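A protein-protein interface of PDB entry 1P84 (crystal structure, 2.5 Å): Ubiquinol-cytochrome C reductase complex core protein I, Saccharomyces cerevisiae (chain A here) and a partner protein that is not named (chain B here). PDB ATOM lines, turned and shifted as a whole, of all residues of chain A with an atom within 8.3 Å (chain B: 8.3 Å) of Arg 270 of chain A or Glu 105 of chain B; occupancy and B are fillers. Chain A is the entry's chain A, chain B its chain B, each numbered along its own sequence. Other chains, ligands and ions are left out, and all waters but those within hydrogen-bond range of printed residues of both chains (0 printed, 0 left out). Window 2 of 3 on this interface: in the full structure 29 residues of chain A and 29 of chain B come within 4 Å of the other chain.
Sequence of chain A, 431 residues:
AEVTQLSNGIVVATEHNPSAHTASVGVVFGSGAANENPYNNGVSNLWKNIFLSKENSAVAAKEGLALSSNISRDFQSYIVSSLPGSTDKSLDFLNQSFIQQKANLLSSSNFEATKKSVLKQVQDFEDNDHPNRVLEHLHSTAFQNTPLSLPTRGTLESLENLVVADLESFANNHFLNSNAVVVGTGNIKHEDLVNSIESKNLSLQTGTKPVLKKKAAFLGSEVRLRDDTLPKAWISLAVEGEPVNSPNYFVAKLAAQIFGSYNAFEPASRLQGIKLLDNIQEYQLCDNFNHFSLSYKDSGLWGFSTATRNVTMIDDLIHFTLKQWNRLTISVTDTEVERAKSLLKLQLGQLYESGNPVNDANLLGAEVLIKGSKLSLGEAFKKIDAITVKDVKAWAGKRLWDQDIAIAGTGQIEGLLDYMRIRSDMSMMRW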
ATOM      1  N   SER A 261     -34.581 -27.910 -27.964  1.00  0.00           N
ATOM      2  CA  SER A 261     -33.834 -28.952 -27.272  1.00  0.00           C
ATOM      3  C   SER A 261     -32.337 -28.715 -27.394  1.00  0.00           C
ATOM      4  O   SER A 261     -31.874 -28.053 -28.328  1.00  0.00           O
ATOM      5  CB  SER A 261     -34.224 -30.354 -27.764  1.00  0.00           C
ATOM      6  OG  SER A 261     -33.768 -30.631 -29.076  1.00  0.00           O
ATOM      7  N   TYR A 262     -31.579 -29.275 -26.456  1.00  0.00           N
ATOM      8  CA  TYR A 262     -30.141 -29.067 -26.423  1.00  0.00           C
ATOM      9  C   TYR A 262     -29.383 -30.283 -25.920  1.00  0.00           C
ATOM     10  O   TYR A 262     -29.890 -31.043 -25.115  1.00  0.00           O
ATOM     11  CB  TYR A 262     -29.859 -27.826 -25.550  1.00  0.00           C
ATOM     12  CG  TYR A 262     -28.456 -27.671 -25.003  1.00  0.00           C
ATOM     13  CD1 TYR A 262     -28.151 -28.072 -23.703  1.00  0.00           C
ATOM     14  CD2 TYR A 262     -27.447 -27.087 -25.761  1.00  0.00           C
ATOM     15  CE1 TYR A 262     -26.879 -27.896 -23.170  1.00  0.00           C
ATOM     16  CE2 TYR A 262     -26.171 -26.902 -25.238  1.00  0.00           C
ATOM     17  CZ  TYR A 262     -25.898 -27.310 -23.941  1.00  0.00           C
ATOM     18  OH  TYR A 262     -24.641 -27.127 -23.418  1.00  0.00           O
ATOM     19  N   ASN A 263     -28.163 -30.447 -26.414  1.00  0.00           N
ATOM     20  CA  ASN A 263     -27.282 -31.546 -26.041  1.00  0.00           C
ATOM     21  C   ASN A 263     -25.875 -30.935 -25.938  1.00  0.00           C
ATOM     22  O   ASN A 263     -25.200 -30.722 -26.944  1.00  0.00           O
ATOM     23  CB  ASN A 263     -27.338 -32.638 -27.113  1.00  0.00           C
ATOM     24  CG  ASN A 263     -26.375 -33.796 -26.857  1.00  0.00           C
ATOM     25  OD1 ASN A 263     -26.565 -34.870 -27.411  1.00  0.00           O
ATOM     26  ND2 ASN A 263     -25.334 -33.578 -26.059  1.00  0.00           N
ATOM     27  N   ALA A 264     -25.440 -30.697 -24.706  1.00  0.00           N
ATOM     28  CA  ALA A 264     -24.146 -30.094 -24.410  1.00  0.00           C
ATOM     29  C   ALA A 264     -22.923 -30.731 -25.046  1.00  0.00           C
ATOM     30  O   ALA A 264     -21.852 -30.132 -25.044  1.00  0.00           O
ATOM     31  CB  ALA A 264     -23.954 -30.021 -22.909  1.00  0.00           C
ATOM     32  N   PHE A 265     -23.055 -31.945 -25.564  1.00  0.00           N
ATOM     33  CA  PHE A 265     -21.903 -32.616 -26.174  1.00  0.00           C
ATOM     34  C   PHE A 265     -21.783 -32.436 -27.692  1.00  0.00           C
ATOM     35  O   PHE A 265     -20.693 -32.576 -28.257  1.00  0.00           O
ATOM     36  CB  PHE A 265     -21.885 -34.092 -25.781  1.00  0.00           C
ATOM     37  CG  PHE A 265     -21.778 -34.312 -24.301  1.00  0.00           C
ATOM     38  CD1 PHE A 265     -22.917 -34.516 -23.530  1.00  0.00           C
ATOM     39  CD2 PHE A 265     -20.540 -34.280 -23.669  1.00  0.00           C
ATOM     40  CE1 PHE A 265     -22.825 -34.683 -22.146  1.00  0.00           C
ATOM     41  CE2 PHE A 265     -20.437 -34.446 -22.288  1.00  0.00           C
ATOM     42  CZ  PHE A 265     -21.584 -34.649 -21.526  1.00  0.00           C
ATOM     43  N   GLU A 266     -22.905 -32.126 -28.340  1.00  0.00           N
ATOM     44  CA  GLU A 266     -22.930 -31.901 -29.779  1.00  0.00           C
ATOM     45  C   GLU A 266     -22.610 -30.434 -30.089  1.00  0.00           C
ATOM     46  O   GLU A 266     -23.447 -29.552 -29.889  1.00  0.00           O
ATOM     47  CB  GLU A 266     -24.302 -32.281 -30.350  1.00  0.00           C
ATOM     48  CG  GLU A 266     -24.559 -33.786 -30.435  1.00  0.00           C
ATOM     49  CD  GLU A 266     -23.654 -34.498 -31.441  1.00  0.00           C
ATOM     50  OE1 GLU A 266     -23.371 -35.698 -31.251  1.00  0.00           O
ATOM     51  OE2 GLU A 266     -23.230 -33.861 -32.431  1.00  0.00           O
ATOM     52  N   PRO A 267     -21.408 -30.165 -30.633  1.00  0.00           N
ATOM     53  CA  PRO A 267     -20.932 -28.820 -30.990  1.00  0.00           C
ATOM     54  C   PRO A 267     -21.956 -27.862 -31.612  1.00  0.00           C
ATOM     55  O   PRO A 267     -22.051 -26.692 -31.219  1.00  0.00           O
ATOM     56  CB  PRO A 267     -19.788 -29.121 -31.948  1.00  0.00           C
ATOM     57  CG  PRO A 267     -19.183 -30.345 -31.329  1.00  0.00           C
ATOM     58  CD  PRO A 267     -20.411 -31.184 -31.015  1.00  0.00           C
ATOM     59  N   ALA A 268     -22.740 -28.363 -32.557  1.00  0.00           N
ATOM     60  CA  ALA A 268     -23.733 -27.535 -33.230  1.00  0.00           C
ATOM     61  C   ALA A 268     -24.851 -27.106 -32.308  1.00  0.00           C
ATOM     62  O   ALA A 268     -25.414 -26.030 -32.479  1.00  0.00           O
ATOM     63  CB  ALA A 268     -24.311 -28.271 -34.442  1.00  0.00           C
ATOM     64  N   SER A 269     -25.184 -27.962 -31.344  1.00  0.00           N
ATOM     65  CA  SER A 269     -26.264 -27.692 -30.395  1.00  0.00           C
ATOM     66  C   SER A 269     -25.926 -26.473 -29.546  1.00  0.00           C
ATOM     67  O   SER A 269     -26.791 -25.650 -29.248  1.00  0.00           O
ATOM     68  CB  SER A 269     -26.491 -28.912 -29.495  1.00  0.00           C
ATOM     69  OG  SER A 269     -27.777 -28.889 -28.897  1.00  0.00           O
ATOM     70  N   ARG A 270     -24.647 -26.343 -29.209  1.00  0.00           N
ATOM     71  CA  ARG A 270     -24.171 -25.232 -28.397  1.00  0.00           C
ATOM     72  C   ARG A 270     -24.268 -23.886 -29.120  1.00  0.00           C
ATOM     73  O   ARG A 270     -24.307 -22.831 -28.476  1.00  0.00           O
ATOM     74  CB  ARG A 270     -22.720 -25.474 -27.954  1.00  0.00           C
ATOM     75  CG  ARG A 270     -22.501 -26.789 -27.206  1.00  0.00           C
ATOM     76  CD  ARG A 270     -21.260 -26.750 -26.311  1.00  0.00           C
ATOM     77  NE  ARG A 270     -20.024 -26.677 -27.081  1.00  0.00           N
ATOM     78  CZ  ARG A 270     -19.166 -27.688 -27.233  1.00  0.00           C
ATOM     79  NH1 ARG A 270     -18.058 -27.529 -27.960  1.00  0.00           N
ATOM     80  NH2 ARG A 270     -19.412 -28.863 -26.664  1.00  0.00           N
ATOM     81  N   LEU A 271     -24.352 -23.925 -30.451  1.00  0.00           N
ATOM     82  CA  LEU A 271     -24.403 -22.707 -31.260  1.00  0.00           C
ATOM     83  C   LEU A 271     -25.787 -22.169 -31.596  1.00  0.00           C
ATOM     84  O   LEU A 271     -25.912 -21.068 -32.128  1.00  0.00           O
ATOM     85  CB  LEU A 271     -23.600 -22.915 -32.538  1.00  0.00           C
ATOM     86  CG  LEU A 271     -22.144 -23.296 -32.267  1.00  0.00           C
ATOM     87  CD1 LEU A 271     -21.437 -23.761 -33.546  1.00  0.00           C
ATOM     88  CD2 LEU A 271     -21.434 -22.115 -31.643  1.00  0.00           C
ATOM     89  N   GLN A 272     -26.823 -22.919 -31.250  1.00  0.00           N
ATOM     90  CA  GLN A 272     -28.196 -22.517 -31.542  1.00  0.00           C
ATOM     91  C   GLN A 272     -28.595 -21.135 -31.060  1.00  0.00           C
ATOM     92  O   GLN A 272     -28.078 -20.644 -30.059  1.00  0.00           O
ATOM     93  CB  GLN A 272     -29.175 -23.524 -30.964  1.00  0.00           C
ATOM     94  CG  GLN A 272     -29.007 -24.934 -31.453  1.00  0.00           C
ATOM     95  CD  GLN A 272     -29.977 -25.844 -30.765  1.00  0.00           C
ATOM     96  OE1 GLN A 272     -31.191 -25.751 -30.980  1.00  0.00           O
ATOM     97  NE2 GLN A 272     -29.463 -26.696 -29.881  1.00  0.00           N
ATOM     98  N   GLY A 273     -29.602 -20.566 -31.720  1.00  0.00           N
ATOM     99  CA  GLY A 273     -30.085 -19.240 -31.384  1.00  0.00           C
ATOM    100  C   GLY A 273     -31.113 -19.213 -30.277  1.00  0.00           C
ATOM    101  O   GLY A 273     -32.236 -18.740 -30.471  1.00  0.00           O
ATOM    102  N   ILE A 274     -30.727 -19.734 -29.117  1.00  0.00           N
ATOM    103  CA  ILE A 274     -31.596 -19.776 -27.937  1.00  0.00           C
ATOM    104  C   ILE A 274     -30.886 -18.965 -26.864  1.00  0.00           C
ATOM    105  O   ILE A 274     -29.753 -19.279 -26.493  1.00  0.00           O
ATOM    106  CB  ILE A 274     -31.781 -21.233 -27.425  1.00  0.00           C
ATOM    107  CG1 ILE A 274     -32.236 -22.143 -28.578  1.00  0.00           C
ATOM    108  CG2 ILE A 274     -32.824 -21.271 -26.297  1.00  0.00           C
ATOM    109  CD1 ILE A 274     -32.058 -23.620 -28.307  1.00  0.00           C
ATOM    110  N   LEU A 277     -29.130 -20.497 -23.672  1.00  0.00           N
ATOM    111  CA  LEU A 277     -27.808 -21.111 -23.740  1.00  0.00           C
ATOM    112  C   LEU A 277     -26.680 -20.234 -23.229  1.00  0.00           C
ATOM    113  O   LEU A 277     -25.619 -20.736 -22.864  1.00  0.00           O
ATOM    114  CB  LEU A 277     -27.498 -21.617 -25.149  1.00  0.00           C
ATOM    115  CG  LEU A 277     -28.377 -22.743 -25.700  1.00  0.00           C
ATOM    116  CD1 LEU A 277     -27.731 -23.313 -26.959  1.00  0.00           C
ATOM    117  CD2 LEU A 277     -28.542 -23.842 -24.673  1.00  0.00           C
ATOM    118  N   ASP A 278     -26.899 -18.924 -23.220  1.00  0.00           N
ATOM    119  CA  ASP A 278     -25.881 -17.998 -22.727  1.00  0.00           C
ATOM    120  C   ASP A 278     -25.731 -18.193 -21.212  1.00  0.00           C
ATOM    121  O   ASP A 278     -24.615 -18.192 -20.686  1.00  0.00           O
ATOM    122  CB  ASP A 278     -26.263 -16.539 -23.044  1.00  0.00           C
ATOM    123  CG  ASP A 278     -26.150 -16.199 -24.536  1.00  0.00           C
ATOM    124  OD1 ASP A 278     -26.985 -15.406 -25.040  1.00  0.00           O
ATOM    125  OD2 ASP A 278     -25.221 -16.709 -25.198  1.00  0.00           O
ATOM    126  N   ILE A 280     -26.880 -21.079 -19.296  1.00  0.00           N
ATOM    127  CA  ILE A 280     -26.556 -22.422 -18.837  1.00  0.00           C
ATOM    128  C   ILE A 280     -25.169 -22.938 -19.180  1.00  0.00           C
ATOM    129  O   ILE A 280     -24.639 -23.783 -18.473  1.00  0.00           O
ATOM    130  CB  ILE A 280     -27.670 -23.472 -19.224  1.00  0.00           C
ATOM    131  CG1 ILE A 280     -27.482 -24.015 -20.635  1.00  0.00           C
ATOM    132  CG2 ILE A 280     -29.053 -22.877 -19.093  1.00  0.00           C
ATOM    133  CD1 ILE A 280     -26.618 -25.273 -20.676  1.00  0.00           C
ATOM    134  N   GLN A 281     -24.545 -22.384 -20.211  1.00  0.00           N
ATOM    135  CA  GLN A 281     -23.224 -22.858 -20.629  1.00  0.00           C
ATOM    136  C   GLN A 281     -22.007 -22.391 -19.847  1.00  0.00           C
ATOM    137  O   GLN A 281     -20.957 -23.037 -19.893  1.00  0.00           O
ATOM    138  CB  GLN A 281     -23.023 -22.615 -22.118  1.00  0.00           C
ATOM    139  CG  GLN A 281     -24.024 -23.385 -22.955  1.00  0.00           C
ATOM    140  CD  GLN A 281     -23.619 -23.492 -24.404  1.00  0.00           C
ATOM    141  OE1 GLN A 281     -23.017 -24.484 -24.812  1.00  0.00           O
ATOM    142  NE2 GLN A 281     -23.949 -22.476 -25.190  1.00  0.00           N
ATOM    143  N   GLN A 284     -21.936 -24.907 -17.102  1.00  0.00           N
ATOM    144  CA  GLN A 284     -22.415 -26.184 -17.606  1.00  0.00           C
ATOM    145  C   GLN A 284     -23.465 -26.763 -16.658  1.00  0.00           C
ATOM    146  O   GLN A 284     -23.230 -27.737 -15.948  1.00  0.00           O
ATOM    147  CB  GLN A 284     -21.253 -27.156 -17.845  1.00  0.00           C
ATOM    148  CG  GLN A 284     -21.629 -28.322 -18.797  1.00  0.00           C
ATOM    149  CD  GLN A 284     -22.187 -27.850 -20.163  1.00  0.00           C
ATOM    150  OE1 GLN A 284     -21.435 -27.679 -21.130  1.00  0.00           O
ATOM    151  NE2 GLN A 284     -23.507 -27.641 -20.232  1.00  0.00           N
ATOM    152  N   GLN B  41     -17.471 -27.247 -39.001  1.00  0.00           N
ATOM    153  CA  GLN B  41     -16.777 -26.334 -38.104  1.00  0.00           C
ATOM    154  C   GLN B  41     -16.634 -25.035 -38.913  1.00  0.00           C
ATOM    155  O   GLN B  41     -17.568 -24.628 -39.619  1.00  0.00           O
ATOM    156  CB  GLN B  41     -15.397 -26.877 -37.723  1.00  0.00           C
ATOM    157  CG  GLN B  41     -15.404 -27.846 -36.558  1.00  0.00           C
ATOM    158  CD  GLN B  41     -15.876 -27.205 -35.257  1.00  0.00           C
ATOM    159  OE1 GLN B  41     -16.738 -27.746 -34.566  1.00  0.00           O
ATOM    160  NE2 GLN B  41     -15.307 -26.053 -34.916  1.00  0.00           N
ATOM    161  N   LEU B  49     -20.874 -20.823 -36.331  1.00  0.00           N
ATOM    162  CA  LEU B  49     -21.956 -20.092 -35.694  1.00  0.00           C
ATOM    163  C   LEU B  49     -22.917 -19.478 -36.719  1.00  0.00           C
ATOM    164  O   LEU B  49     -24.135 -19.648 -36.609  1.00  0.00           O
ATOM    165  CB  LEU B  49     -21.375 -19.006 -34.769  1.00  0.00           C
ATOM    166  CG  LEU B  49     -22.289 -17.959 -34.122  1.00  0.00           C
ATOM    167  CD1 LEU B  49     -23.302 -18.600 -33.202  1.00  0.00           C
ATOM    168  CD2 LEU B  49     -21.430 -16.981 -33.367  1.00  0.00           C
ATOM    169  N   VAL B  52     -25.060 -22.106 -38.559  1.00  0.00           N
ATOM    170  CA  VAL B  52     -26.189 -22.578 -37.772  1.00  0.00           C
ATOM    171  C   VAL B  52     -27.292 -21.530 -37.648  1.00  0.00           C
ATOM    172  O   VAL B  52     -28.472 -21.822 -37.848  1.00  0.00           O
ATOM    173  CB  VAL B  52     -25.747 -23.030 -36.351  1.00  0.00           C
ATOM    174  CG1 VAL B  52     -26.946 -23.513 -35.552  1.00  0.00           C
ATOM    175  CG2 VAL B  52     -24.689 -24.120 -36.430  1.00  0.00           C
ATOM    176  N   ARG B  53     -26.913 -20.299 -37.339  1.00  0.00           N
ATOM    177  CA  ARG B  53     -27.907 -19.248 -37.172  1.00  0.00           C
ATOM    178  C   ARG B  53     -28.680 -19.037 -38.456  1.00  0.00           C
ATOM    179  O   ARG B  53     -29.889 -18.849 -38.418  1.00  0.00           O
ATOM    180  CB  ARG B  53     -27.257 -17.946 -36.693  1.00  0.00           C
ATOM    181  CG  ARG B  53     -26.374 -18.128 -35.466  1.00  0.00           C
ATOM    182  CD  ARG B  53     -27.141 -18.739 -34.292  1.00  0.00           C
ATOM    183  NE  ARG B  53     -27.747 -17.720 -33.443  1.00  0.00           N
ATOM    184  CZ  ARG B  53     -27.245 -17.325 -32.279  1.00  0.00           C
ATOM    185  NH1 ARG B  53     -27.864 -16.384 -31.586  1.00  0.00           N
ATOM    186  NH2 ARG B  53     -26.147 -17.891 -31.794  1.00  0.00           N
ATOM    187  N   GLU B  56     -31.054 -22.107 -39.423  1.00  0.00           N
ATOM    188  CA  GLU B  56     -32.190 -22.137 -38.510  1.00  0.00           C
ATOM    189  C   GLU B  56     -33.274 -21.188 -38.998  1.00  0.00           C
ATOM    190  O   GLU B  56     -34.457 -21.517 -38.956  1.00  0.00           O
ATOM    191  CB  GLU B  56     -31.768 -21.736 -37.098  1.00  0.00           C
ATOM    192  CG  GLU B  56     -30.948 -22.780 -36.352  1.00  0.00           C
ATOM    193  CD  GLU B  56     -30.603 -22.372 -34.917  1.00  0.00           C
ATOM    194  OE1 GLU B  56     -30.985 -21.265 -34.472  1.00  0.00           O
ATOM    195  OE2 GLU B  56     -29.955 -23.181 -34.231  1.00  0.00           O
ATOM    196  N   LYS B  99      -8.642 -24.638 -37.900  1.00  0.00           N
ATOM    197  CA  LYS B  99      -7.873 -23.824 -36.956  1.00  0.00           C
ATOM    198  C   LYS B  99      -7.428 -24.672 -35.763  1.00  0.00           C
ATOM    199  O   LYS B  99      -8.217 -25.423 -35.203  1.00  0.00           O
ATOM    200  CB  LYS B  99      -8.709 -22.635 -36.483  1.00  0.00           C
ATOM    201  CG  LYS B  99      -9.208 -21.732 -37.611  1.00  0.00           C
ATOM    202  CD  LYS B  99      -8.063 -21.021 -38.331  1.00  0.00           C
ATOM    203  CE  LYS B  99      -7.728 -19.674 -37.698  1.00  0.00           C
ATOM    204  NZ  LYS B  99      -8.765 -18.641 -37.999  1.00  0.00           N
ATOM    205  N   PRO B 100      -6.156 -24.556 -35.353  1.00  0.00           N
ATOM    206  CA  PRO B 100      -5.599 -25.314 -34.224  1.00  0.00           C
ATOM    207  C   PRO B 100      -6.461 -25.277 -32.954  1.00  0.00           C
ATOM    208  O   PRO B 100      -6.487 -26.241 -32.187  1.00  0.00           O
ATOM    209  CB  PRO B 100      -4.253 -24.625 -33.986  1.00  0.00           C
ATOM    210  CG  PRO B 100      -3.874 -24.165 -35.331  1.00  0.00           C
ATOM    211  CD  PRO B 100      -5.166 -23.601 -35.872  1.00  0.00           C
ATOM    212  N   HIS B 101      -7.167 -24.167 -32.740  1.00  0.00           N
ATOM    213  CA  HIS B 101      -8.008 -24.039 -31.563  1.00  0.00           C
ATOM    214  C   HIS B 101      -9.334 -24.785 -31.669  1.00  0.00           C
ATOM    215  O   HIS B 101      -9.929 -25.137 -30.649  1.00  0.00           O
ATOM    216  CB  HIS B 101      -8.229 -22.569 -31.191  1.00  0.00           C
ATOM    217  CG  HIS B 101      -9.172 -21.828 -32.091  1.00  0.00           C
ATOM    218  ND1 HIS B 101      -8.741 -20.906 -33.022  1.00  0.00           N
ATOM    219  CD2 HIS B 101     -10.526 -21.813 -32.149  1.00  0.00           C
ATOM    220  CE1 HIS B 101      -9.788 -20.354 -33.608  1.00  0.00           C
ATOM    221  NE2 HIS B 101     -10.883 -20.887 -33.097  1.00  0.00           N
ATOM    222  N   GLU B 102      -9.807 -25.013 -32.891  1.00  0.00           N
ATOM    223  CA  GLU B 102     -11.061 -25.737 -33.089  1.00  0.00           C
ATOM    224  C   GLU B 102     -10.858 -27.209 -32.773  1.00  0.00           C
ATOM    225  O   GLU B 102     -11.787 -27.896 -32.351  1.00  0.00           O
ATOM    226  CB  GLU B 102     -11.558 -25.575 -34.519  1.00  0.00           C
ATOM    227  CG  GLU B 102     -11.780 -24.142 -34.899  1.00  0.00           C
ATOM    228  CD  GLU B 102     -12.492 -24.010 -36.210  1.00  0.00           C
ATOM    229  OE1 GLU B 102     -11.805 -24.026 -37.259  1.00  0.00           O
ATOM    230  OE2 GLU B 102     -13.738 -23.900 -36.186  1.00  0.00           O
ATOM    231  N   LEU B 103      -9.628 -27.680 -32.961  1.00  0.00           N
ATOM    232  CA  LEU B 103      -9.300 -29.067 -32.683  1.00  0.00           C
ATOM    233  C   LEU B 103      -9.384 -29.319 -31.183  1.00  0.00           C
ATOM    234  O   LEU B 103     -10.116 -30.207 -30.738  1.00  0.00           O
ATOM    235  CB  LEU B 103      -7.895 -29.408 -33.190  1.00  0.00           C
ATOM    236  CG  LEU B 103      -7.495 -30.872 -32.981  1.00  0.00           C
ATOM    237  CD1 LEU B 103      -8.476 -31.774 -33.724  1.00  0.00           C
ATOM    238  CD2 LEU B 103      -6.065 -31.119 -33.435  1.00  0.00           C
ATOM    239  N   THR B 104      -8.661 -28.507 -30.410  1.00  0.00           N
ATOM    240  CA  THR B 104      -8.632 -28.635 -28.951  1.00  0.00           C
ATOM    241  C   THR B 104      -9.936 -28.279 -28.230  1.00  0.00           C
ATOM    242  O   THR B 104     -10.282 -28.898 -27.228  1.00  0.00           O
ATOM    243  CB  THR B 104      -7.496 -27.794 -28.335  1.00  0.00           C
ATOM    244  OG1 THR B 104      -7.601 -26.452 -28.807  1.00  0.00           O
ATOM    245  CG2 THR B 104      -6.135 -28.341 -28.722  1.00  0.00           C
ATOM    246  N   GLU B 105     -10.687 -27.335 -28.777  1.00  0.00           N
ATOM    247  CA  GLU B 105     -11.922 -26.889 -28.146  1.00  0.00           C
ATOM    248  C   GLU B 105     -13.224 -27.550 -28.561  1.00  0.00           C
ATOM    249  O   GLU B 105     -14.158 -27.595 -27.766  1.00  0.00           O
ATOM    250  CB  GLU B 105     -12.064 -25.371 -28.291  1.00  0.00           C
ATOM    251  CG  GLU B 105     -10.917 -24.585 -27.662  1.00  0.00           C
ATOM    252  CD  GLU B 105     -11.028 -23.087 -27.875  1.00  0.00           C
ATOM    253  OE1 GLU B 105     -12.115 -22.616 -28.294  1.00  0.00           O
ATOM    254  OE2 GLU B 105     -10.022 -22.383 -27.619  1.00  0.00           O
ATOM    255  N   SER B 106     -13.309 -28.047 -29.793  1.00  0.00           N
ATOM    256  CA  SER B 106     -14.550 -28.667 -30.257  1.00  0.00           C
ATOM    257  C   SER B 106     -14.428 -30.092 -30.776  1.00  0.00           C
ATOM    258  O   SER B 106     -15.207 -30.961 -30.385  1.00  0.00           O
ATOM    259  CB  SER B 106     -15.209 -27.804 -31.332  1.00  0.00           C
ATOM    260  OG  SER B 106     -15.402 -26.475 -30.884  1.00  0.00           O
ATOM    261  N   VAL B 107     -13.447 -30.332 -31.638  1.00  0.00           N
ATOM    262  CA  VAL B 107     -13.255 -31.648 -32.234  1.00  0.00           C
ATOM    263  C   VAL B 107     -12.850 -32.746 -31.258  1.00  0.00           C
ATOM    264  O   VAL B 107     -13.597 -33.710 -31.070  1.00  0.00           O
ATOM    265  CB  VAL B 107     -12.269 -31.578 -33.434  1.00  0.00           C
ATOM    266  CG1 VAL B 107     -12.029 -32.967 -34.017  1.00  0.00           C
ATOM    267  CG2 VAL B 107     -12.837 -30.657 -34.510  1.00  0.00           C
ATOM    268  N   LEU B 108     -11.677 -32.618 -30.648  1.00  0.00           N
ATOM    269  CA  LEU B 108     -11.216 -33.621 -29.697  1.00  0.00           C
ATOM    270  C   LEU B 108     -12.279 -33.964 -28.638  1.00  0.00           C
ATOM    271  O   LEU B 108     -12.527 -35.129 -28.373  1.00  0.00           O
ATOM    272  CB  LEU B 108      -9.903 -33.179 -29.058  1.00  0.00           C
ATOM    273  CG  LEU B 108      -8.703 -33.233 -30.000  1.00  0.00           C
ATOM    274  CD1 LEU B 108      -7.512 -32.493 -29.404  1.00  0.00           C
ATOM    275  CD2 LEU B 108      -8.346 -34.685 -30.289  1.00  0.00           C
ATOM    276  N   PRO B 109     -12.902 -32.950 -28.003  1.00  0.00           N
ATOM    277  CA  PRO B 109     -13.930 -33.241 -26.997  1.00  0.00           C
ATOM    278  C   PRO B 109     -15.068 -34.080 -27.576  1.00  0.00           C
ATOM    279  O   PRO B 109     -15.422 -35.118 -27.023  1.00  0.00           O
ATOM    280  CB  PRO B 109     -14.419 -31.845 -26.605  1.00  0.00           C
ATOM    281  CG  PRO B 109     -13.163 -31.055 -26.664  1.00  0.00           C
ATOM    282  CD  PRO B 109     -12.550 -31.515 -27.970  1.00  0.00           C
ATOM    283  N   ALA B 110     -15.629 -33.632 -28.696  1.00  0.00           N
ATOM    284  CA  ALA B 110     -16.728 -34.344 -29.346  1.00  0.00           C
ATOM    285  C   ALA B 110     -16.316 -35.780 -29.649  1.00  0.00           C
ATOM    286  O   ALA B 110     -17.097 -36.710 -29.463  1.00  0.00           O
ATOM    287  CB  ALA B 110     -17.139 -33.629 -30.625  1.00  0.00           C
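Of the printed residues of chain B, Pro 267 of chain A touches Ala 110 (3.9 Å).
Ala 268 of chain A touches none of the printed residues of chain B.
Of the printed residues of chain B, Arg 270 of chain A touches Glu 105.
Printed residues of chain B within 4 Å of Gly 273 of chain A: Arg 53 (3.5 Å) and Glu 56 (3.2 Å).
Of the printed residues of chain A, Leu 49 of chain B touches Leu 271.
Glu 102 of chain B touches none of the printed residues of chain A.
Glu 105 of chain B touches one residue of chain A.
The nearest residue of chain B that does not touch Arg 270 of chain A is Ser 106 of chain B (4.1 Å).
The nearest residue of chain A that does not touch Glu 105 of chain B is Pro 267 of chain A (6.7 Å).
The nearest printed residue of chain A that does not touch Glu 56 of chain B is Leu 271 of chain A (5.0 Å).
Hydrophobic or aromatic side chains of chain A that line the printed part of chain B: Pro 267.
Of the 17 printed residues of chain B, 5 touch a printed residue of chain A.
Printed residues of chain B that touch a printed residue of chain A: Leu 49, Arg 53, Glu 56, Glu 105 and Ala 110.
Hydrophobic or aromatic side chains of chain B within 4 Å of the printed part of chain A: Leu 49 and Ala 110.
Among the printed residues, 8 pairs touch across the chains.
Among the printed residues, no Asp or Glu carboxylate lies within 4 Å of a Lys or Arg side-chain nitrogen of the other chain.
O of Leu 271 of chain A is in hydrogen-bond range of NH2 of Arg 53 of chain B, 3.2 Å away.
N of Gly 273 of chain A is in hydrogen-bond range of OE1 of Glu 56 of chain B (3.2 Å).
Ala 110 of chain B touches Pro 267 of chain A (CB to CG, 3.9 Å).
NH1 of Arg 270 of chain A touches O of Glu 105 of chain B (3.9 Å).
Leu 271 of chain A touches Leu 49 of chain B (O to CD1, 3.7 Å).
Gln 272 of chain A touches Arg 53 of chain B (O to NH2, 3.8 Å).
CA of Gln 272 of chain A touches OE2 of Glu 56 of chain B, 3.3 Å away.
NE of Arg 53 of chain B touches CA of Gly 273 of chain A, 3.5 Å away.
The backbone carbonyl oxygen (O) of Ser 261 of chain A lies within hydrogen-bond range of the side-chain amide nitrogen (NE2) of Gln 272 of chain A (3.2 Å).
The backbone carbonyl oxygen (O) of Ala 264 of chain A sits at hydrogen-bond distance from the guanidinium group (NH2) of Arg 270 of chain A.
OG of Ser 269 of chain A sits at hydrogen-bond distance from NE2 of Gln 272 of chain A (2.9 Å).
The backbone carbonyl oxygen of Arg 270 of chain A is in hydrogen-bond range of the side-chain amide nitrogen of Gln 281 of chain A.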
